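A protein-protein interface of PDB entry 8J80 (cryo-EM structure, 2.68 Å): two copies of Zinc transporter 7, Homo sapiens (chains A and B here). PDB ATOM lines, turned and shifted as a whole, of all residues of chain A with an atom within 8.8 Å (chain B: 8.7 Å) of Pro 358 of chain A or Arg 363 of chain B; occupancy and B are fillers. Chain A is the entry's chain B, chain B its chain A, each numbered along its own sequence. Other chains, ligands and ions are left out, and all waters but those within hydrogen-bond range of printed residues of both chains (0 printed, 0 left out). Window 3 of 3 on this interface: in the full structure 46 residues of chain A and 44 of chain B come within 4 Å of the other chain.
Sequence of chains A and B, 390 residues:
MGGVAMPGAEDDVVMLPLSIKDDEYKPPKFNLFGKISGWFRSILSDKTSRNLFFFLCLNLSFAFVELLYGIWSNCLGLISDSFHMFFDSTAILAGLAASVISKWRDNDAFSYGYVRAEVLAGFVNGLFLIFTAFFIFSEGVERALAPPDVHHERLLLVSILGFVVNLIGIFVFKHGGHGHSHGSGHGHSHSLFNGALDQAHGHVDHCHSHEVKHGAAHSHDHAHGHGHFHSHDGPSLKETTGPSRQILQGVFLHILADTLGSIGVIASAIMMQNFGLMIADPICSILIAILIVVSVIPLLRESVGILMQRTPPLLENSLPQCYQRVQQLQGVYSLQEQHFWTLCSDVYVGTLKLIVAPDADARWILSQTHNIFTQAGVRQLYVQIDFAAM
The backbone carbonyl oxygen of Pro 358 of chain A lies within hydrogen-bond range of the guanidinium group of Arg 363 of chain B (2.9 Å).
A ring nitrogen (ND1) of His 370 of chain B sits at hydrogen-bond distance from the backbone carbonyl oxygen (O) of Leu 366 of chain B (3.4 Å). The backbone NH (N) of Val 356 of chain A lies within hydrogen-bond range of the backbone carbonyl oxygen (O) of Asp 386 of chain A, 2.9 Å away. The side-chain carboxylate of Asp 386 of chain A sits at hydrogen-bond distance from the side-chain amide nitrogen of Gln 384 of chain A.
Among the printed residues, pairs that only touch across the chains: Gln 384 of chain A with Leu 366 of chain B (3.8 Å), Gln 384 of chain A with His 370 of chain B (3.0 Å), Ile 385 of chain A with Leu 366 of chain B (3.5 Å), Asp 386 of chain A with Leu 366 of chain B (3.2 Å) and Phe 387 of chain A with Arg 363 of chain B (3.6 Å).
No residue of chain B comes within 4 Å of Ala 357 of chain A. Asp 359 of chain A touches none of the printed residues of chain B. Of the printed residues of chain B, Gln 384 of chain A touches Leu 366 (3.8 Å) and His 370 (3.0 Å). Of the printed residues of chain B, Ile 385 of chain A touches Leu 366. Of the printed residues of chain A, Leu 366 of chain B touches Gln 384, Ile 385 and Asp 386. The nearest printed residue of chain B that does not touch Pro 358 of chain A is Asp 361 of chain B (9.7 Å). The nearest printed residue of chain A that does not touch Arg 363 of chain B is Asp 359 of chain A (5.0 Å). The nearest printed residue of chain A that does not touch Leu 366 of chain B is Phe 387 of chain A (6.0 Å).
Of the 15 printed residues of chain B, 3 touch a printed residue of chain A. Hydrophobic or aromatic side chains of chain B that line the printed part of chain A: Leu 366 and His 370. Hydrophobic or aromatic side chains of chain A within 4 Å of the printed part of chain B: Phe 387. Among the printed residues, no Asp or Glu carboxylate lies within 4 Å of a Lys or Arg side-chain nitrogen of the other chain.
Positions printed for both chains: 356, 360, 361, 362, 385 and 387. Of the 6 pairs that touch across the chains among the printed residues, none has its exchanged pair printed and touching as well.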
ATOM      1  N   GLY A 331      10.132  15.644  18.777  1.00  0.00           N
ATOM      2  CA  GLY A 331       9.714  16.271  20.002  1.00  0.00           C
ATOM      3  C   GLY A 331       8.274  16.043  20.370  1.00  0.00           C
ATOM      4  O   GLY A 331       7.854  16.478  21.440  1.00  0.00           O
ATOM      5  N   VAL A 332       7.503  15.383  19.521  1.00  0.00           N
ATOM      6  CA  VAL A 332       6.130  15.024  19.838  1.00  0.00           C
ATOM      7  C   VAL A 332       6.143  13.688  20.555  1.00  0.00           C
ATOM      8  O   VAL A 332       6.731  12.717  20.073  1.00  0.00           O
ATOM      9  CB  VAL A 332       5.259  14.971  18.572  1.00  0.00           C
ATOM     10  CG1 VAL A 332       3.896  14.375  18.886  1.00  0.00           C
ATOM     11  CG2 VAL A 332       5.100  16.363  17.980  1.00  0.00           C
ATOM     12  N   TYR A 333       5.511  13.643  21.721  1.00  0.00           N
ATOM     13  CA  TYR A 333       5.397  12.436  22.516  1.00  0.00           C
ATOM     14  C   TYR A 333       4.126  11.668  22.183  1.00  0.00           C
ATOM     15  O   TYR A 333       4.190  10.473  21.892  1.00  0.00           O
ATOM     16  CB  TYR A 333       5.443  12.790  24.007  1.00  0.00           C
ATOM     17  CG  TYR A 333       6.805  13.204  24.530  1.00  0.00           C
ATOM     18  CD1 TYR A 333       7.903  13.296  23.692  1.00  0.00           C
ATOM     19  CD2 TYR A 333       6.986  13.491  25.873  1.00  0.00           C
ATOM     20  CE1 TYR A 333       9.125  13.667  24.167  1.00  0.00           C
ATOM     21  CE2 TYR A 333       8.215  13.861  26.365  1.00  0.00           C
ATOM     22  CZ  TYR A 333       9.283  13.943  25.511  1.00  0.00           C
ATOM     23  OH  TYR A 333      10.516  14.314  25.992  1.00  0.00           O
ATOM     24  N   ILE A 355       1.091  16.269  23.296  1.00  0.00           N
ATOM     25  CA  ILE A 355       2.093  16.313  24.347  1.00  0.00           C
ATOM     26  C   ILE A 355       3.442  16.315  23.656  1.00  0.00           C
ATOM     27  O   ILE A 355       3.668  15.533  22.731  1.00  0.00           O
ATOM     28  CB  ILE A 355       1.951  15.129  25.319  1.00  0.00           C
ATOM     29  CG1 ILE A 355       0.550  15.124  25.929  1.00  0.00           C
ATOM     30  CG2 ILE A 355       2.997  15.216  26.413  1.00  0.00           C
ATOM     31  CD1 ILE A 355       0.349  14.110  27.010  1.00  0.00           C
ATOM     32  N   VAL A 356       4.317  17.232  24.048  1.00  0.00           N
ATOM     33  CA  VAL A 356       5.612  17.363  23.405  1.00  0.00           C
ATOM     34  C   VAL A 356       6.705  17.329  24.464  1.00  0.00           C
ATOM     35  O   VAL A 356       6.442  17.308  25.665  1.00  0.00           O
ATOM     36  CB  VAL A 356       5.723  18.639  22.538  1.00  0.00           C
ATOM     37  CG1 VAL A 356       4.694  18.615  21.396  1.00  0.00           C
ATOM     38  CG2 VAL A 356       5.596  19.893  23.387  1.00  0.00           C
ATOM     39  N   ALA A 357       7.945  17.329  23.991  1.00  0.00           N
ATOM     40  CA  ALA A 357       9.093  17.346  24.875  1.00  0.00           C
ATOM     41  C   ALA A 357       9.117  18.631  25.701  1.00  0.00           C
ATOM     42  O   ALA A 357       8.617  19.672  25.268  1.00  0.00           O
ATOM     43  CB  ALA A 357      10.373  17.219  24.064  1.00  0.00           C
ATOM     44  N   PRO A 358       9.690  18.585  26.907  1.00  0.00           N
ATOM     45  CA  PRO A 358       9.756  19.795  27.738  1.00  0.00           C
ATOM     46  C   PRO A 358      10.563  20.933  27.128  1.00  0.00           C
ATOM     47  O   PRO A 358      10.478  22.058  27.631  1.00  0.00           O
ATOM     48  CB  PRO A 358      10.399  19.291  29.036  1.00  0.00           C
ATOM     49  CG  PRO A 358      10.995  17.981  28.694  1.00  0.00           C
ATOM     50  CD  PRO A 358      10.125  17.398  27.654  1.00  0.00           C
ATOM     51  N   ASP A 359      11.333  20.683  26.069  1.00  0.00           N
ATOM     52  CA  ASP A 359      12.097  21.727  25.398  1.00  0.00           C
ATOM     53  C   ASP A 359      11.797  21.793  23.905  1.00  0.00           C
ATOM     54  O   ASP A 359      12.572  22.392  23.160  1.00  0.00           O
ATOM     55  CB  ASP A 359      13.599  21.522  25.626  1.00  0.00           C
ATOM     56  CG  ASP A 359      14.118  20.210  25.041  1.00  0.00           C
ATOM     57  OD1 ASP A 359      13.390  19.197  25.081  1.00  0.00           O
ATOM     58  OD2 ASP A 359      15.271  20.192  24.566  1.00  0.00           O
ATOM     59  N   ALA A 360      10.675  21.232  23.459  1.00  0.00           N
ATOM     60  CA  ALA A 360      10.430  21.055  22.032  1.00  0.00           C
ATOM     61  C   ALA A 360      10.109  22.372  21.327  1.00  0.00           C
ATOM     62  O   ALA A 360       9.606  23.326  21.923  1.00  0.00           O
ATOM     63  CB  ALA A 360       9.296  20.058  21.799  1.00  0.00           C
ATOM     64  N   ASP A 361      10.412  22.403  20.032  1.00  0.00           N
ATOM     65  CA  ASP A 361      10.133  23.525  19.147  1.00  0.00           C
ATOM     66  C   ASP A 361       8.645  23.599  18.840  1.00  0.00           C
ATOM     67  O   ASP A 361       8.167  22.944  17.915  1.00  0.00           O
ATOM     68  CB  ASP A 361      10.949  23.380  17.860  1.00  0.00           C
ATOM     69  CG  ASP A 361      11.063  24.668  17.070  1.00  0.00           C
ATOM     70  OD1 ASP A 361      10.394  25.672  17.389  1.00  0.00           O
ATOM     71  OD2 ASP A 361      11.831  24.669  16.096  1.00  0.00           O
ATOM     72  N   ALA A 362       7.912  24.400  19.613  1.00  0.00           N
ATOM     73  CA  ALA A 362       6.464  24.486  19.480  1.00  0.00           C
ATOM     74  C   ALA A 362       6.029  25.247  18.234  1.00  0.00           C
ATOM     75  O   ALA A 362       5.007  24.896  17.637  1.00  0.00           O
ATOM     76  CB  ALA A 362       5.864  25.138  20.725  1.00  0.00           C
ATOM     77  N   GLN A 384      -3.741  22.348  20.508  1.00  0.00           N
ATOM     78  CA  GLN A 384      -3.230  22.697  21.822  1.00  0.00           C
ATOM     79  C   GLN A 384      -1.971  21.883  22.075  1.00  0.00           C
ATOM     80  O   GLN A 384      -1.936  20.688  21.788  1.00  0.00           O
ATOM     81  CB  GLN A 384      -4.270  22.438  22.907  1.00  0.00           C
ATOM     82  CG  GLN A 384      -3.735  22.594  24.315  1.00  0.00           C
ATOM     83  CD  GLN A 384      -4.828  22.599  25.344  1.00  0.00           C
ATOM     84  OE1 GLN A 384      -5.855  23.229  25.158  1.00  0.00           O
ATOM     85  NE2 GLN A 384      -4.613  21.893  26.434  1.00  0.00           N
ATOM     86  N   ILE A 385      -0.928  22.540  22.564  1.00  0.00           N
ATOM     87  CA  ILE A 385       0.359  21.911  22.814  1.00  0.00           C
ATOM     88  C   ILE A 385       0.653  21.993  24.303  1.00  0.00           C
ATOM     89  O   ILE A 385       0.630  23.081  24.887  1.00  0.00           O
ATOM     90  CB  ILE A 385       1.471  22.567  21.978  1.00  0.00           C
ATOM     91  CG1 ILE A 385       1.330  22.153  20.510  1.00  0.00           C
ATOM     92  CG2 ILE A 385       2.847  22.203  22.511  1.00  0.00           C
ATOM     93  CD1 ILE A 385       1.952  23.116  19.537  1.00  0.00           C
ATOM     94  N   ASP A 386       0.907  20.842  24.916  1.00  0.00           N
ATOM     95  CA  ASP A 386       1.278  20.730  26.317  1.00  0.00           C
ATOM     96  C   ASP A 386       2.691  20.180  26.410  1.00  0.00           C
ATOM     97  O   ASP A 386       3.008  19.170  25.781  1.00  0.00           O
ATOM     98  CB  ASP A 386       0.319  19.811  27.073  1.00  0.00           C
ATOM     99  CG  ASP A 386      -1.126  20.227  26.931  1.00  0.00           C
ATOM    100  OD1 ASP A 386      -1.807  19.761  25.990  1.00  0.00           O
ATOM    101  OD2 ASP A 386      -1.588  21.019  27.775  1.00  0.00           O
ATOM    102  N   PHE A 387       3.526  20.831  27.204  1.00  0.00           N
ATOM    103  CA  PHE A 387       4.885  20.373  27.432  1.00  0.00           C
ATOM    104  C   PHE A 387       4.898  19.370  28.575  1.00  0.00           C
ATOM    105  O   PHE A 387       4.245  19.572  29.601  1.00  0.00           O
ATOM    106  CB  PHE A 387       5.808  21.553  27.735  1.00  0.00           C
ATOM    107  CG  PHE A 387       5.956  22.509  26.590  1.00  0.00           C
ATOM    108  CD1 PHE A 387       5.025  23.507  26.383  1.00  0.00           C
ATOM    109  CD2 PHE A 387       7.019  22.406  25.712  1.00  0.00           C
ATOM    110  CE1 PHE A 387       5.152  24.383  25.320  1.00  0.00           C
ATOM    111  CE2 PHE A 387       7.150  23.276  24.652  1.00  0.00           C
ATOM    112  CZ  PHE A 387       6.217  24.264  24.458  1.00  0.00           C
ATOM    113  N   ALA A 388       5.618  18.274  28.374  1.00  0.00           N
ATOM    114  CA  ALA A 388       5.693  17.223  29.372  1.00  0.00           C
ATOM    115  C   ALA A 388       6.668  17.601  30.481  1.00  0.00           C
ATOM    116  O   ALA A 388       7.467  18.529  30.358  1.00  0.00           O
ATOM    117  CB  ALA A 388       6.107  15.907  28.726  1.00  0.00           C
ATOM    118  N   ALA A 389       6.586  16.874  31.594  1.00  0.00           N
ATOM    119  CA  ALA A 389       7.550  17.068  32.670  1.00  0.00           C
ATOM    120  C   ALA A 389       8.907  16.460  32.329  1.00  0.00           C
ATOM    121  O   ALA A 389       9.948  17.080  32.569  1.00  0.00           O
ATOM    122  CB  ALA A 389       7.009  16.475  33.967  1.00  0.00           C
ATOM    123  N   MET A 390       8.914  15.258  31.765  1.00  0.00           N
ATOM    124  CA  MET A 390      10.149  14.543  31.463  1.00  0.00           C
ATOM    125  C   MET A 390      10.174  14.052  30.022  1.00  0.00           C
ATOM    126  O   MET A 390       9.318  13.273  29.615  1.00  0.00           O
ATOM    127  CB  MET A 390      10.325  13.362  32.425  1.00  0.00           C
ATOM    128  CG  MET A 390      11.299  12.290  31.949  1.00  0.00           C
ATOM    129  SD  MET A 390      12.977  12.519  32.544  1.00  0.00           S
ATOM    130  CE  MET A 390      12.974  11.458  33.983  1.00  0.00           C
ATOM    131  N   VAL B 356       0.575  35.362  21.759  1.00  0.00           N
ATOM    132  CA  VAL B 356       1.315  35.711  22.959  1.00  0.00           C
ATOM    133  C   VAL B 356       2.643  36.334  22.555  1.00  0.00           C
ATOM    134  O   VAL B 356       3.030  36.328  21.389  1.00  0.00           O
ATOM    135  CB  VAL B 356       1.534  34.499  23.895  1.00  0.00           C
ATOM    136  CG1 VAL B 356       0.202  33.976  24.431  1.00  0.00           C
ATOM    137  CG2 VAL B 356       2.305  33.407  23.186  1.00  0.00           C
ATOM    138  N   ALA B 360       6.840  34.285  26.078  1.00  0.00           N
ATOM    139  CA  ALA B 360       5.862  34.178  27.149  1.00  0.00           C
ATOM    140  C   ALA B 360       5.841  32.779  27.757  1.00  0.00           C
ATOM    141  O   ALA B 360       6.198  31.790  27.118  1.00  0.00           O
ATOM    142  CB  ALA B 360       4.470  34.549  26.641  1.00  0.00           C
ATOM    143  N   ASP B 361       5.420  32.715  29.019  1.00  0.00           N
ATOM    144  CA  ASP B 361       5.218  31.467  29.744  1.00  0.00           C
ATOM    145  C   ASP B 361       3.960  30.773  29.245  1.00  0.00           C
ATOM    146  O   ASP B 361       2.870  30.994  29.778  1.00  0.00           O
ATOM    147  CB  ASP B 361       5.120  31.744  31.247  1.00  0.00           C
ATOM    148  CG  ASP B 361       5.429  30.532  32.098  1.00  0.00           C
ATOM    149  OD1 ASP B 361       5.444  29.402  31.585  1.00  0.00           O
ATOM    150  OD2 ASP B 361       5.666  30.712  33.303  1.00  0.00           O
ATOM    151  N   ALA B 362       4.107  29.935  28.218  1.00  0.00           N
ATOM    152  CA  ALA B 362       2.952  29.298  27.594  1.00  0.00           C
ATOM    153  C   ALA B 362       2.310  28.261  28.503  1.00  0.00           C
ATOM    154  O   ALA B 362       1.093  28.077  28.452  1.00  0.00           O
ATOM    155  CB  ALA B 362       3.359  28.666  26.263  1.00  0.00           C
ATOM    156  N   ARG B 363       3.110  27.567  29.321  1.00  0.00           N
ATOM    157  CA  ARG B 363       2.566  26.630  30.299  1.00  0.00           C
ATOM    158  C   ARG B 363       1.609  27.334  31.249  1.00  0.00           C
ATOM    159  O   ARG B 363       0.483  26.873  31.487  1.00  0.00           O
ATOM    160  CB  ARG B 363       3.699  25.985  31.094  1.00  0.00           C
ATOM    161  CG  ARG B 363       4.558  24.988  30.363  1.00  0.00           C
ATOM    162  CD  ARG B 363       5.703  24.562  31.260  1.00  0.00           C
ATOM    163  NE  ARG B 363       6.696  23.734  30.590  1.00  0.00           N
ATOM    164  CZ  ARG B 363       7.658  24.189  29.800  1.00  0.00           C
ATOM    165  NH1 ARG B 363       7.768  25.473  29.514  1.00  0.00           N
ATOM    166  NH2 ARG B 363       8.530  23.333  29.282  1.00  0.00           N
ATOM    167  N   TRP B 364       2.043  28.469  31.791  1.00  0.00           N
ATOM    168  CA  TRP B 364       1.227  29.183  32.755  1.00  0.00           C
ATOM    169  C   TRP B 364       0.002  29.808  32.092  1.00  0.00           C
ATOM    170  O   TRP B 364      -1.089  29.802  32.670  1.00  0.00           O
ATOM    171  CB  TRP B 364       2.080  30.233  33.472  1.00  0.00           C
ATOM    172  CG  TRP B 364       1.288  31.071  34.377  1.00  0.00           C
ATOM    173  CD1 TRP B 364       0.896  30.769  35.637  1.00  0.00           C
ATOM    174  CD2 TRP B 364       0.734  32.350  34.078  1.00  0.00           C
ATOM    175  NE1 TRP B 364       0.149  31.785  36.153  1.00  0.00           N
ATOM    176  CE2 TRP B 364       0.037  32.774  35.216  1.00  0.00           C
ATOM    177  CE3 TRP B 364       0.774  33.186  32.962  1.00  0.00           C
ATOM    178  CZ2 TRP B 364      -0.622  33.990  35.269  1.00  0.00           C
ATOM    179  CZ3 TRP B 364       0.120  34.380  33.015  1.00  0.00           C
ATOM    180  CH2 TRP B 364      -0.571  34.777  34.159  1.00  0.00           C
ATOM    181  N   ILE B 365       0.165  30.352  30.885  1.00  0.00           N
ATOM    182  CA  ILE B 365      -0.958  30.946  30.167  1.00  0.00           C
ATOM    183  C   ILE B 365      -2.005  29.885  29.858  1.00  0.00           C
ATOM    184  O   ILE B 365      -3.213  30.128  29.971  1.00  0.00           O
ATOM    185  CB  ILE B 365      -0.465  31.655  28.888  1.00  0.00           C
ATOM    186  CG1 ILE B 365       0.142  33.017  29.219  1.00  0.00           C
ATOM    187  CG2 ILE B 365      -1.586  31.825  27.892  1.00  0.00           C
ATOM    188  CD1 ILE B 365       0.892  33.653  28.090  1.00  0.00           C
ATOM    189  N   LEU B 366      -1.556  28.689  29.484  1.00  0.00           N
ATOM    190  CA  LEU B 366      -2.473  27.589  29.216  1.00  0.00           C
ATOM    191  C   LEU B 366      -3.235  27.181  30.471  1.00  0.00           C
ATOM    192  O   LEU B 366      -4.459  27.007  30.437  1.00  0.00           O
ATOM    193  CB  LEU B 366      -1.689  26.410  28.637  1.00  0.00           C
ATOM    194  CG  LEU B 366      -2.442  25.237  28.011  1.00  0.00           C
ATOM    195  CD1 LEU B 366      -3.330  25.687  26.876  1.00  0.00           C
ATOM    196  CD2 LEU B 366      -1.450  24.210  27.527  1.00  0.00           C
ATOM    197  N   SER B 367      -2.528  27.038  31.594  1.00  0.00           N
ATOM    198  CA  SER B 367      -3.196  26.651  32.833  1.00  0.00           C
ATOM    199  C   SER B 367      -4.198  27.708  33.280  1.00  0.00           C
ATOM    200  O   SER B 367      -5.291  27.380  33.760  1.00  0.00           O
ATOM    201  CB  SER B 367      -2.159  26.373  33.923  1.00  0.00           C
ATOM    202  OG  SER B 367      -1.584  27.561  34.420  1.00  0.00           O
ATOM    203  N   GLN B 368      -3.861  28.984  33.097  1.00  0.00           N
ATOM    204  CA  GLN B 368      -4.757  30.064  33.497  1.00  0.00           C
ATOM    205  C   GLN B 368      -5.981  30.153  32.600  1.00  0.00           C
ATOM    206  O   GLN B 368      -7.089  30.391  33.087  1.00  0.00           O
ATOM    207  CB  GLN B 368      -4.004  31.385  33.496  1.00  0.00           C
ATOM    208  CG  GLN B 368      -2.988  31.475  34.577  1.00  0.00           C
ATOM    209  CD  GLN B 368      -3.600  31.485  35.950  1.00  0.00           C
ATOM    210  OE1 GLN B 368      -3.440  30.544  36.723  1.00  0.00           O
ATOM    211  NE2 GLN B 368      -4.304  32.558  36.266  1.00  0.00           N
ATOM    212  N   THR B 369      -5.804  29.988  31.288  1.00  0.00           N
ATOM    213  CA  THR B 369      -6.944  30.005  30.376  1.00  0.00           C
ATOM    214  C   THR B 369      -7.886  28.848  30.664  1.00  0.00           C
ATOM    215  O   THR B 369      -9.117  29.010  30.656  1.00  0.00           O
ATOM    216  CB  THR B 369      -6.448  29.964  28.924  1.00  0.00           C
ATOM    217  OG1 THR B 369      -5.557  31.056  28.695  1.00  0.00           O
ATOM    218  CG2 THR B 369      -7.593  30.072  27.943  1.00  0.00           C
ATOM    219  N   HIS B 370      -7.324  27.676  30.949  1.00  0.00           N
ATOM    220  CA  HIS B 370      -8.160  26.527  31.256  1.00  0.00           C
ATOM    221  C   HIS B 370      -8.896  26.710  32.575  1.00  0.00           C
ATOM    222  O   HIS B 370     -10.053  26.305  32.698  1.00  0.00           O
ATOM    223  CB  HIS B 370      -7.315  25.262  31.249  1.00  0.00           C
ATOM    224  CG  HIS B 370      -7.375  24.523  29.953  1.00  0.00           C
ATOM    225  ND1 HIS B 370      -6.598  24.860  28.868  1.00  0.00           N
ATOM    226  CD2 HIS B 370      -8.148  23.487  29.553  1.00  0.00           C
ATOM    227  CE1 HIS B 370      -6.878  24.053  27.863  1.00  0.00           C
ATOM    228  NE2 HIS B 370      -7.815  23.211  28.252  1.00  0.00           N
ATOM    229  N   ASN B 371      -8.258  27.339  33.562  1.00  0.00           N
ATOM    230  CA  ASN B 371      -8.962  27.682  34.792  1.00  0.00           C
ATOM    231  C   ASN B 371     -10.104  28.658  34.532  1.00  0.00           C
ATOM    232  O   ASN B 371     -11.216  28.484  35.050  1.00  0.00           O
ATOM    233  CB  ASN B 371      -7.980  28.272  35.798  1.00  0.00           C
ATOM    234  CG  ASN B 371      -7.309  27.219  36.625  1.00  0.00           C
ATOM    235  OD1 ASN B 371      -6.084  27.107  36.639  1.00  0.00           O
ATOM    236  ND2 ASN B 371      -8.107  26.429  37.327  1.00  0.00           N
ATOM    237  N   ILE B 385      -1.813  28.275  21.156  1.00  0.00           N
ATOM    238  CA  ILE B 385      -0.947  29.392  21.497  1.00  0.00           C
ATOM    239  C   ILE B 385      -0.001  29.629  20.328  1.00  0.00           C
ATOM    240  O   ILE B 385       0.691  28.709  19.881  1.00  0.00           O
ATOM    241  CB  ILE B 385      -0.201  29.121  22.813  1.00  0.00           C
ATOM    242  CG1 ILE B 385      -1.171  29.283  23.988  1.00  0.00           C
ATOM    243  CG2 ILE B 385       0.993  30.030  22.970  1.00  0.00           C
ATOM    244  CD1 ILE B 385      -0.884  28.397  25.165  1.00  0.00           C
ATOM    245  N   PHE B 387       3.121  32.124  19.116  1.00  0.00           N
ATOM    246  CA  PHE B 387       4.111  33.102  19.552  1.00  0.00           C
ATOM    247  C   PHE B 387       4.264  34.190  18.501  1.00  0.00           C
ATOM    248  O   PHE B 387       4.365  33.902  17.307  1.00  0.00           O
ATOM    249  CB  PHE B 387       5.450  32.422  19.830  1.00  0.00           C
ATOM    250  CG  PHE B 387       5.431  31.536  21.031  1.00  0.00           C
ATOM    251  CD1 PHE B 387       5.713  32.042  22.282  1.00  0.00           C
ATOM    252  CD2 PHE B 387       5.100  30.202  20.916  1.00  0.00           C
ATOM    253  CE1 PHE B 387       5.681  31.235  23.390  1.00  0.00           C
ATOM    254  CE2 PHE B 387       5.061  29.391  22.025  1.00  0.00           C
ATOM    255  CZ  PHE B 387       5.353  29.908  23.260  1.00  0.00           C
